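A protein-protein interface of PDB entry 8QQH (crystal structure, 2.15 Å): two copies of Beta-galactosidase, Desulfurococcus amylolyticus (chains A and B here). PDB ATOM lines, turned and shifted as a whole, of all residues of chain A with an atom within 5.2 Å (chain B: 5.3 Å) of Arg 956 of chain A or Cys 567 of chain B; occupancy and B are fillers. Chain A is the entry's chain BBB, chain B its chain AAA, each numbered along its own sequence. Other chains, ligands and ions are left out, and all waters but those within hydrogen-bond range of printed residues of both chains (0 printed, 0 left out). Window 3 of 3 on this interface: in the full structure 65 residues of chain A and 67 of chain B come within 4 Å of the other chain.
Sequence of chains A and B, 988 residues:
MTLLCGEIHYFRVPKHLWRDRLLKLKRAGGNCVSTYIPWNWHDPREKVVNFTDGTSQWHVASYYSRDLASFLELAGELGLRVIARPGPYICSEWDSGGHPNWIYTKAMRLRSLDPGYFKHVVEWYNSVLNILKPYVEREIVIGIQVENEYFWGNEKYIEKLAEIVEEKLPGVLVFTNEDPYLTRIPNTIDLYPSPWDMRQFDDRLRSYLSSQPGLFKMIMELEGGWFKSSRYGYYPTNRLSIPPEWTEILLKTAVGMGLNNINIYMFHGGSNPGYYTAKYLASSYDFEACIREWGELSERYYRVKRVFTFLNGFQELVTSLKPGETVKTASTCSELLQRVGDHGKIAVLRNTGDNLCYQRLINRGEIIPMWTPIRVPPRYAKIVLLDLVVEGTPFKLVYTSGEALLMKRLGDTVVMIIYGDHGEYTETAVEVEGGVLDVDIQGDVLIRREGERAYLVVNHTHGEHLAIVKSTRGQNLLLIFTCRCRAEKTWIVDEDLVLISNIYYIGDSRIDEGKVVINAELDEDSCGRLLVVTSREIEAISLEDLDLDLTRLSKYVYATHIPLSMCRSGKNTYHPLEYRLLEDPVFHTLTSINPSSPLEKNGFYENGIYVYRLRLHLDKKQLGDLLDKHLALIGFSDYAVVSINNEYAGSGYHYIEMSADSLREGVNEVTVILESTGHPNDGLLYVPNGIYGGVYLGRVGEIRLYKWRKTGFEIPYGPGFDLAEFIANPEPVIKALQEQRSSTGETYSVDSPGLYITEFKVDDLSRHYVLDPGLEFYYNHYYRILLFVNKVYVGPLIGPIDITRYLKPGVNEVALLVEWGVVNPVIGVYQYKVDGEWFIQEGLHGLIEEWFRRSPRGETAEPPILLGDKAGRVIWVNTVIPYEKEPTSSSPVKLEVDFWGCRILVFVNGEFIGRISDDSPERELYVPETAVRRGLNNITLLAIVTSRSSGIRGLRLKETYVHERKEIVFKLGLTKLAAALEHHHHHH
The side-chain carboxylate (OD1) of Asp 525 of chain B lies within salt-bridge range of the guanidinium group (NH2) of Arg 956 of chain A. O of Glu 524 of chain B lies within hydrogen-bond range of NH1 of Arg 956 of chain A (2.7 Å).
SG of Cys 567 of chain B forms a disulfide with SG of Cys 527 of chain B (2.1 Å). The side-chain carboxylate (OD1) of Asp 523 of chain B lies close to the backbone NH (N) of Asp 525 of chain B (3.2 Å). OE1 of Glu 896 of chain A is in salt-bridge range of NH2 of Arg 956 of chain A, 2.8 Å away. The side-chain sulfur of Cys 567 of chain B is in hydrogen-bond range of the backbone NH of Ser 526 of chain B, at 3.7 Å. The side-chain carboxylate of Glu 524 of chain B is in hydrogen-bond range of the side-chain hydroxyl of Ser 569 of chain B (2.9 Å).
OG1 of Thr 573 of chain A touches CB of Ser 569 of chain B, at 3.7 Å. Gly 954 of chain A touches Leu 564 of chain B. Leu 955 of chain A touches Leu 564 of chain B. Arg 956 of chain A touches Cys 567 of chain B (NH1 to O, 3.9 Å).
Of the printed residues of chain B, Leu 955 of chain A touches Leu 564 (3.7 Å). Of chain B, only Glu 524, Asp 525 and Cys 567 come within 4 Å of Arg 956 of chain A. Of the printed residues of chain A, Leu 564 of chain B touches Gly 954 and Leu 955. The nearest residue of chain B that does not touch Arg 956 of chain A is Leu 564 of chain B (4.2 Å). The nearest printed residue of chain A that does not touch Cys 567 of chain B is His 575 of chain A (5.2 Å).
Printed residues of chain B that touch a printed residue of chain A: Glu 524, Asp 525, Leu 564, Cys 567 and Ser 569. Hydrophobic or aromatic side chains of chain B that line the printed part of chain A: Leu 564. Among the printed residues, 6 pairs touch across the chains. Among the printed residues, Asp or Glu carboxylates within 4 Å of a Lys or Arg side-chain nitrogen of the other chain: Arg 956 of chain A with Asp 525 of chain B (3.2 Å).
No position is printed for both chains. Of the 6 pairs that touch across the chains among the printed residues, none has its exchanged pair printed and touching as well.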
ATOM      1  N   THR A 573      -3.581 -26.570  -0.476  1.00  0.00           N
ATOM      2  CA  THR A 573      -3.295 -26.411   0.972  1.00  0.00           C
ATOM      3  C   THR A 573      -3.529 -24.949   1.359  1.00  0.00           C
ATOM      4  O   THR A 573      -3.249 -24.091   0.544  1.00  0.00           O
ATOM      5  CB  THR A 573      -1.863 -26.839   1.275  1.00  0.00           C
ATOM      6  OG1 THR A 573      -1.801 -28.200   0.866  1.00  0.00           O
ATOM      7  CG2 THR A 573      -1.503 -26.708   2.734  1.00  0.00           C
ATOM      8  N   TYR A 574      -4.010 -24.673   2.565  1.00  0.00           N
ATOM      9  CA  TYR A 574      -4.369 -23.298   3.006  1.00  0.00           C
ATOM     10  C   TYR A 574      -3.670 -23.028   4.335  1.00  0.00           C
ATOM     11  O   TYR A 574      -3.866 -23.806   5.294  1.00  0.00           O
ATOM     12  CB  TYR A 574      -5.887 -23.103   3.088  1.00  0.00           C
ATOM     13  CG  TYR A 574      -6.650 -23.431   1.831  1.00  0.00           C
ATOM     14  CD1 TYR A 574      -7.006 -24.744   1.553  1.00  0.00           C
ATOM     15  CD2 TYR A 574      -7.034 -22.448   0.923  1.00  0.00           C
ATOM     16  CE1 TYR A 574      -7.675 -25.083   0.385  1.00  0.00           C
ATOM     17  CE2 TYR A 574      -7.722 -22.772  -0.244  1.00  0.00           C
ATOM     18  CZ  TYR A 574      -8.036 -24.097  -0.520  1.00  0.00           C
ATOM     19  OH  TYR A 574      -8.744 -24.463  -1.633  1.00  0.00           O
ATOM     20  N   HIS A 575      -2.888 -21.949   4.389  1.00  0.00           N
ATOM     21  CA  HIS A 575      -1.956 -21.602   5.492  1.00  0.00           C
ATOM     22  C   HIS A 575      -2.545 -20.491   6.359  1.00  0.00           C
ATOM     23  O   HIS A 575      -3.266 -19.653   5.859  1.00  0.00           O
ATOM     24  CB  HIS A 575      -0.587 -21.286   4.873  1.00  0.00           C
ATOM     25  CG  HIS A 575      -0.015 -22.484   4.185  1.00  0.00           C
ATOM     26  ND1 HIS A 575      -0.153 -22.694   2.818  1.00  0.00           N
ATOM     27  CD2 HIS A 575       0.630 -23.572   4.667  1.00  0.00           C
ATOM     28  CE1 HIS A 575       0.416 -23.841   2.492  1.00  0.00           C
ATOM     29  NE2 HIS A 575       0.919 -24.391   3.601  1.00  0.00           N
ATOM     30  N   PRO A 576      -2.329 -20.490   7.696  1.00  0.00           N
ATOM     31  CA  PRO A 576      -2.790 -19.393   8.550  1.00  0.00           C
ATOM     32  C   PRO A 576      -2.143 -18.044   8.202  1.00  0.00           C
ATOM     33  O   PRO A 576      -1.057 -18.028   7.757  1.00  0.00           O
ATOM     34  CB  PRO A 576      -2.371 -19.795   9.968  1.00  0.00           C
ATOM     35  CG  PRO A 576      -1.382 -20.927   9.793  1.00  0.00           C
ATOM     36  CD  PRO A 576      -1.714 -21.573   8.473  1.00  0.00           C
ATOM     37  N   ILE A 881      -7.566 -18.671   8.621  1.00  0.00           N
ATOM     38  CA  ILE A 881      -7.206 -19.325   7.330  1.00  0.00           C
ATOM     39  C   ILE A 881      -8.199 -18.882   6.272  1.00  0.00           C
ATOM     40  O   ILE A 881      -9.399 -19.072   6.423  1.00  0.00           O
ATOM     41  CB  ILE A 881      -7.138 -20.855   7.454  1.00  0.00           C
ATOM     42  CG1 ILE A 881      -6.139 -21.264   8.540  1.00  0.00           C
ATOM     43  CG2 ILE A 881      -6.809 -21.458   6.098  1.00  0.00           C
ATOM     44  CD1 ILE A 881      -5.925 -22.756   8.670  1.00  0.00           C
ATOM     45  N   LYS A 894      -9.093 -31.495   5.611  1.00  0.00           N
ATOM     46  CA  LYS A 894      -8.496 -31.982   6.860  1.00  0.00           C
ATOM     47  C   LYS A 894      -7.654 -30.856   7.439  1.00  0.00           C
ATOM     48  O   LYS A 894      -7.028 -30.084   6.664  1.00  0.00           O
ATOM     49  CB  LYS A 894      -7.671 -33.233   6.560  1.00  0.00           C
ATOM     50  CG  LYS A 894      -8.515 -34.423   6.160  1.00  0.00           C
ATOM     51  CD  LYS A 894      -7.703 -35.683   6.036  1.00  0.00           C
ATOM     52  CE  LYS A 894      -8.501 -36.829   5.465  1.00  0.00           C
ATOM     53  NZ  LYS A 894      -7.639 -37.987   5.136  1.00  0.00           N
ATOM     54  N   LEU A 895      -7.634 -30.780   8.756  1.00  0.00           N
ATOM     55  CA  LEU A 895      -6.719 -29.894   9.489  1.00  0.00           C
ATOM     56  C   LEU A 895      -5.589 -30.751  10.041  1.00  0.00           C
ATOM     57  O   LEU A 895      -5.890 -31.690  10.789  1.00  0.00           O
ATOM     58  CB  LEU A 895      -7.485 -29.216  10.617  1.00  0.00           C
ATOM     59  CG  LEU A 895      -6.623 -28.270  11.440  1.00  0.00           C
ATOM     60  CD1 LEU A 895      -6.283 -27.038  10.616  1.00  0.00           C
ATOM     61  CD2 LEU A 895      -7.323 -27.889  12.725  1.00  0.00           C
ATOM     62  N   GLU A 896      -4.350 -30.430   9.701  1.00  0.00           N
ATOM     63  CA  GLU A 896      -3.138 -31.076  10.276  1.00  0.00           C
ATOM     64  C   GLU A 896      -2.460 -30.094  11.225  1.00  0.00           C
ATOM     65  O   GLU A 896      -2.354 -28.908  10.847  1.00  0.00           O
ATOM     66  CB  GLU A 896      -2.177 -31.489   9.173  1.00  0.00           C
ATOM     67  CG  GLU A 896      -0.814 -31.964   9.655  1.00  0.00           C
ATOM     68  CD  GLU A 896       0.003 -32.605   8.542  1.00  0.00           C
ATOM     69  OE1 GLU A 896      -0.127 -32.143   7.373  1.00  0.00           O
ATOM     70  OE2 GLU A 896       0.718 -33.599   8.824  1.00  0.00           O
ATOM     71  N   GLY A 954       3.263 -25.761  13.459  1.00  0.00           N
ATOM     72  CA  GLY A 954       2.337 -25.089  12.541  1.00  0.00           C
ATOM     73  C   GLY A 954       1.107 -25.906  12.284  1.00  0.00           C
ATOM     74  O   GLY A 954       1.001 -27.039  12.821  1.00  0.00           O
ATOM     75  N   LEU A 955       0.183 -25.328  11.531  1.00  0.00           N
ATOM     76  CA  LEU A 955      -1.008 -26.067  11.081  1.00  0.00           C
ATOM     77  C   LEU A 955      -1.384 -25.647   9.647  1.00  0.00           C
ATOM     78  O   LEU A 955      -0.976 -24.535   9.183  1.00  0.00           O
ATOM     79  CB  LEU A 955      -2.120 -25.855  12.120  1.00  0.00           C
ATOM     80  CG  LEU A 955      -2.659 -24.438  12.287  1.00  0.00           C
ATOM     81  CD1 LEU A 955      -3.684 -24.107  11.221  1.00  0.00           C
ATOM     82  CD2 LEU A 955      -3.303 -24.286  13.644  1.00  0.00           C
ATOM     83  N   ARG A 956      -2.121 -26.522   8.959  1.00  0.00           N
ATOM     84  CA  ARG A 956      -2.654 -26.252   7.609  1.00  0.00           C
ATOM     85  C   ARG A 956      -3.987 -26.972   7.399  1.00  0.00           C
ATOM     86  O   ARG A 956      -4.256 -28.001   8.060  1.00  0.00           O
ATOM     87  CB  ARG A 956      -1.583 -26.637   6.582  1.00  0.00           C
ATOM     88  CG  ARG A 956      -1.001 -28.036   6.759  1.00  0.00           C
ATOM     89  CD  ARG A 956       0.039 -28.392   5.702  1.00  0.00           C
ATOM     90  NE  ARG A 956       0.443 -29.793   5.817  1.00  0.00           N
ATOM     91  CZ  ARG A 956       1.447 -30.371   5.154  1.00  0.00           C
ATOM     92  NH1 ARG A 956       2.183 -29.680   4.299  1.00  0.00           N
ATOM     93  NH2 ARG A 956       1.716 -31.649   5.358  1.00  0.00           N
ATOM     94  N   LEU A 957      -4.799 -26.434   6.498  1.00  0.00           N
ATOM     95  CA  LEU A 957      -6.036 -27.065   6.002  1.00  0.00           C
ATOM     96  C   LEU A 957      -5.659 -27.696   4.673  1.00  0.00           C
ATOM     97  O   LEU A 957      -5.068 -26.970   3.859  1.00  0.00           O
ATOM     98  CB  LEU A 957      -7.117 -26.020   5.738  1.00  0.00           C
ATOM     99  CG  LEU A 957      -8.214 -25.820   6.771  1.00  0.00           C
ATOM    100  CD1 LEU A 957      -9.206 -24.785   6.245  1.00  0.00           C
ATOM    101  CD2 LEU A 957      -8.932 -27.121   7.113  1.00  0.00           C
ATOM    102  N   LYS A 958      -6.000 -28.965   4.442  1.00  0.00           N
ATOM    103  CA  LYS A 958      -5.587 -29.679   3.211  1.00  0.00           C
ATOM    104  C   LYS A 958      -6.835 -30.204   2.540  1.00  0.00           C
ATOM    105  O   LYS A 958      -7.632 -30.841   3.226  1.00  0.00           O
ATOM    106  CB  LYS A 958      -4.656 -30.850   3.510  1.00  0.00           C
ATOM    107  CG  LYS A 958      -3.253 -30.483   3.962  1.00  0.00           C
ATOM    108  CD  LYS A 958      -2.369 -31.717   4.222  1.00  0.00           C
ATOM    109  CE  LYS A 958      -2.760 -32.456   5.478  1.00  0.00           C
ATOM    110  NZ  LYS A 958      -2.120 -33.791   5.545  1.00  0.00           N
ATOM    111  N   LEU B 522      12.060 -32.057  -1.115  1.00  0.00           N
ATOM    112  CA  LEU B 522      10.987 -31.916  -0.101  1.00  0.00           C
ATOM    113  C   LEU B 522       9.644 -32.330  -0.721  1.00  0.00           C
ATOM    114  O   LEU B 522       9.301 -31.823  -1.802  1.00  0.00           O
ATOM    115  CB  LEU B 522      10.914 -30.465   0.375  1.00  0.00           C
ATOM    116  CG  LEU B 522      12.208 -29.813   0.845  1.00  0.00           C
ATOM    117  CD1 LEU B 522      11.909 -28.372   1.256  1.00  0.00           C
ATOM    118  CD2 LEU B 522      12.827 -30.567   1.997  1.00  0.00           C
ATOM    119  N   ASP B 523       8.962 -33.271  -0.082  1.00  0.00           N
ATOM    120  CA  ASP B 523       7.539 -33.577  -0.340  1.00  0.00           C
ATOM    121  C   ASP B 523       6.751 -32.699   0.645  1.00  0.00           C
ATOM    122  O   ASP B 523       7.374 -31.871   1.413  1.00  0.00           O
ATOM    123  CB  ASP B 523       7.300 -35.096  -0.290  1.00  0.00           C
ATOM    124  CG  ASP B 523       7.297 -35.731   1.097  1.00  0.00           C
ATOM    125  OD1 ASP B 523       7.670 -35.054   2.088  1.00  0.00           O
ATOM    126  OD2 ASP B 523       6.971 -36.919   1.178  1.00  0.00           O
ATOM    127  N   GLU B 524       5.445 -32.880   0.674  1.00  0.00           N
ATOM    128  CA  GLU B 524       4.532 -32.021   1.469  1.00  0.00           C
ATOM    129  C   GLU B 524       4.707 -32.261   2.977  1.00  0.00           C
ATOM    130  O   GLU B 524       4.227 -31.424   3.743  1.00  0.00           O
ATOM    131  CB  GLU B 524       3.083 -32.250   1.030  1.00  0.00           C
ATOM    132  CG  GLU B 524       2.545 -33.627   1.363  1.00  0.00           C
ATOM    133  CD  GLU B 524       1.102 -33.803   0.924  1.00  0.00           C
ATOM    134  OE1 GLU B 524       0.240 -32.959   1.339  1.00  0.00           O
ATOM    135  OE2 GLU B 524       0.851 -34.756   0.144  1.00  0.00           O
ATOM    136  N   ASP B 525       5.371 -33.341   3.397  1.00  0.00           N
ATOM    137  CA  ASP B 525       5.540 -33.683   4.837  1.00  0.00           C
ATOM    138  C   ASP B 525       6.994 -33.529   5.243  1.00  0.00           C
ATOM    139  O   ASP B 525       7.344 -34.145   6.227  1.00  0.00           O
ATOM    140  CB  ASP B 525       5.118 -35.128   5.160  1.00  0.00           C
ATOM    141  CG  ASP B 525       3.725 -35.467   4.637  1.00  0.00           C
ATOM    142  OD1 ASP B 525       2.832 -34.649   4.807  1.00  0.00           O
ATOM    143  OD2 ASP B 525       3.561 -36.523   4.023  1.00  0.00           O
ATOM    144  N   SER B 526       7.798 -32.769   4.496  1.00  0.00           N
ATOM    145  CA  SER B 526       9.273 -32.746   4.654  1.00  0.00           C
ATOM    146  C   SER B 526       9.699 -31.627   5.600  1.00  0.00           C
ATOM    147  O   SER B 526      10.927 -31.509   5.915  1.00  0.00           O
ATOM    148  CB  SER B 526       9.961 -32.648   3.331  1.00  0.00           C
ATOM    149  OG  SER B 526       9.795 -33.884   2.629  1.00  0.00           O
ATOM    150  N   CYS B 527       8.732 -30.846   6.053  1.00  0.00           N
ATOM    151  CA  CYS B 527       8.983 -29.605   6.819  1.00  0.00           C
ATOM    152  C   CYS B 527       9.064 -29.954   8.304  1.00  0.00           C
ATOM    153  O   CYS B 527       8.801 -31.094   8.637  1.00  0.00           O
ATOM    154  CB  CYS B 527       7.948 -28.558   6.428  1.00  0.00           C
ATOM    155  SG  CYS B 527       8.341 -27.818   4.810  1.00  0.00           S
ATOM    156  N   ILE B 562      12.534 -26.415   9.333  1.00  0.00           N
ATOM    157  CA  ILE B 562      12.094 -25.894   8.010  1.00  0.00           C
ATOM    158  C   ILE B 562      10.661 -25.395   8.182  1.00  0.00           C
ATOM    159  O   ILE B 562       9.782 -26.146   8.613  1.00  0.00           O
ATOM    160  CB  ILE B 562      12.265 -26.981   6.929  1.00  0.00           C
ATOM    161  CG1 ILE B 562      13.737 -27.389   6.825  1.00  0.00           C
ATOM    162  CG2 ILE B 562      11.719 -26.517   5.581  1.00  0.00           C
ATOM    163  CD1 ILE B 562      14.030 -28.381   5.739  1.00  0.00           C
ATOM    164  N   PRO B 563      10.361 -24.111   7.871  1.00  0.00           N
ATOM    165  CA  PRO B 563       8.990 -23.603   8.002  1.00  0.00           C
ATOM    166  C   PRO B 563       7.999 -24.458   7.198  1.00  0.00           C
ATOM    167  O   PRO B 563       8.369 -24.901   6.101  1.00  0.00           O
ATOM    168  CB  PRO B 563       9.052 -22.163   7.461  1.00  0.00           C
ATOM    169  CG  PRO B 563      10.518 -21.797   7.589  1.00  0.00           C
ATOM    170  CD  PRO B 563      11.296 -23.090   7.371  1.00  0.00           C
ATOM    171  N   LEU B 564       6.822 -24.704   7.782  1.00  0.00           N
ATOM    172  CA  LEU B 564       5.741 -25.561   7.229  1.00  0.00           C
ATOM    173  C   LEU B 564       5.239 -24.988   5.880  1.00  0.00           C
ATOM    174  O   LEU B 564       4.778 -25.795   5.027  1.00  0.00           O
ATOM    175  CB  LEU B 564       4.626 -25.721   8.278  1.00  0.00           C
ATOM    176  CG  LEU B 564       3.575 -26.808   7.976  1.00  0.00           C
ATOM    177  CD1 LEU B 564       4.170 -28.224   7.987  1.00  0.00           C
ATOM    178  CD2 LEU B 564       2.401 -26.744   8.947  1.00  0.00           C
ATOM    179  N   SER B 565       5.413 -23.682   5.641  1.00  0.00           N
ATOM    180  CA  SER B 565       5.051 -22.951   4.388  1.00  0.00           C
ATOM    181  C   SER B 565       5.874 -23.405   3.162  1.00  0.00           C
ATOM    182  O   SER B 565       5.355 -23.276   2.026  1.00  0.00           O
ATOM    183  CB  SER B 565       5.164 -21.451   4.605  1.00  0.00           C
ATOM    184  OG  SER B 565       5.904 -21.156   5.791  1.00  0.00           O
ATOM    185  N   MET B 566       7.094 -23.923   3.352  1.00  0.00           N
ATOM    186  CA  MET B 566       8.055 -24.293   2.266  1.00  0.00           C
ATOM    187  C   MET B 566       7.703 -25.635   1.597  1.00  0.00           C
ATOM    188  O   MET B 566       8.439 -26.037   0.656  1.00  0.00           O
ATOM    189  CB  MET B 566       9.479 -24.414   2.824  1.00  0.00           C
ATOM    190  CG  MET B 566      10.052 -23.099   3.314  1.00  0.00           C
ATOM    191  SD  MET B 566      10.646 -22.036   1.963  1.00  0.00           S
ATOM    192  CE  MET B 566      11.015 -20.545   2.889  1.00  0.00           C
ATOM    193  N   CYS B 567       6.678 -26.348   2.076  1.00  0.00           N
ATOM    194  CA  CYS B 567       6.297 -27.706   1.572  1.00  0.00           C
ATOM    195  C   CYS B 567       4.973 -27.660   0.768  1.00  0.00           C
ATOM    196  O   CYS B 567       3.924 -27.926   1.346  1.00  0.00           O
ATOM    197  CB  CYS B 567       6.210 -28.687   2.744  1.00  0.00           C
ATOM    198  SG  CYS B 567       7.819 -29.236   3.388  1.00  0.00           S
ATOM    199  N   ARG B 568       5.015 -27.379  -0.535  1.00  0.00           N
ATOM    200  CA  ARG B 568       3.797 -27.313  -1.396  1.00  0.00           C
ATOM    201  C   ARG B 568       3.271 -28.721  -1.740  1.00  0.00           C
ATOM    202  O   ARG B 568       4.001 -29.714  -1.525  1.00  0.00           O
ATOM    203  CB  ARG B 568       4.073 -26.497  -2.663  1.00  0.00           C
ATOM    204  CG  ARG B 568       3.879 -24.998  -2.479  1.00  0.00           C
ATOM    205  CD  ARG B 568       4.581 -24.158  -3.540  1.00  0.00           C
ATOM    206  NE  ARG B 568       5.080 -22.902  -2.991  1.00  0.00           N
ATOM    207  CZ  ARG B 568       6.117 -22.784  -2.156  1.00  0.00           C
ATOM    208  NH1 ARG B 568       6.791 -23.850  -1.752  1.00  0.00           N
ATOM    209  NH2 ARG B 568       6.474 -21.591  -1.715  1.00  0.00           N
ATOM    210  N   SER B 569       2.039 -28.768  -2.272  1.00  0.00           N
ATOM    211  CA  SER B 569       1.227 -29.967  -2.619  1.00  0.00           C
ATOM    212  C   SER B 569       0.789 -29.945  -4.098  1.00  0.00           C
ATOM    213  O   SER B 569      -0.278 -30.548  -4.403  1.00  0.00           O
ATOM    214  CB  SER B 569       0.016 -30.046  -1.713  1.00  0.00           C
ATOM    215  OG  SER B 569       0.296 -30.840  -0.574  1.00  0.00           O
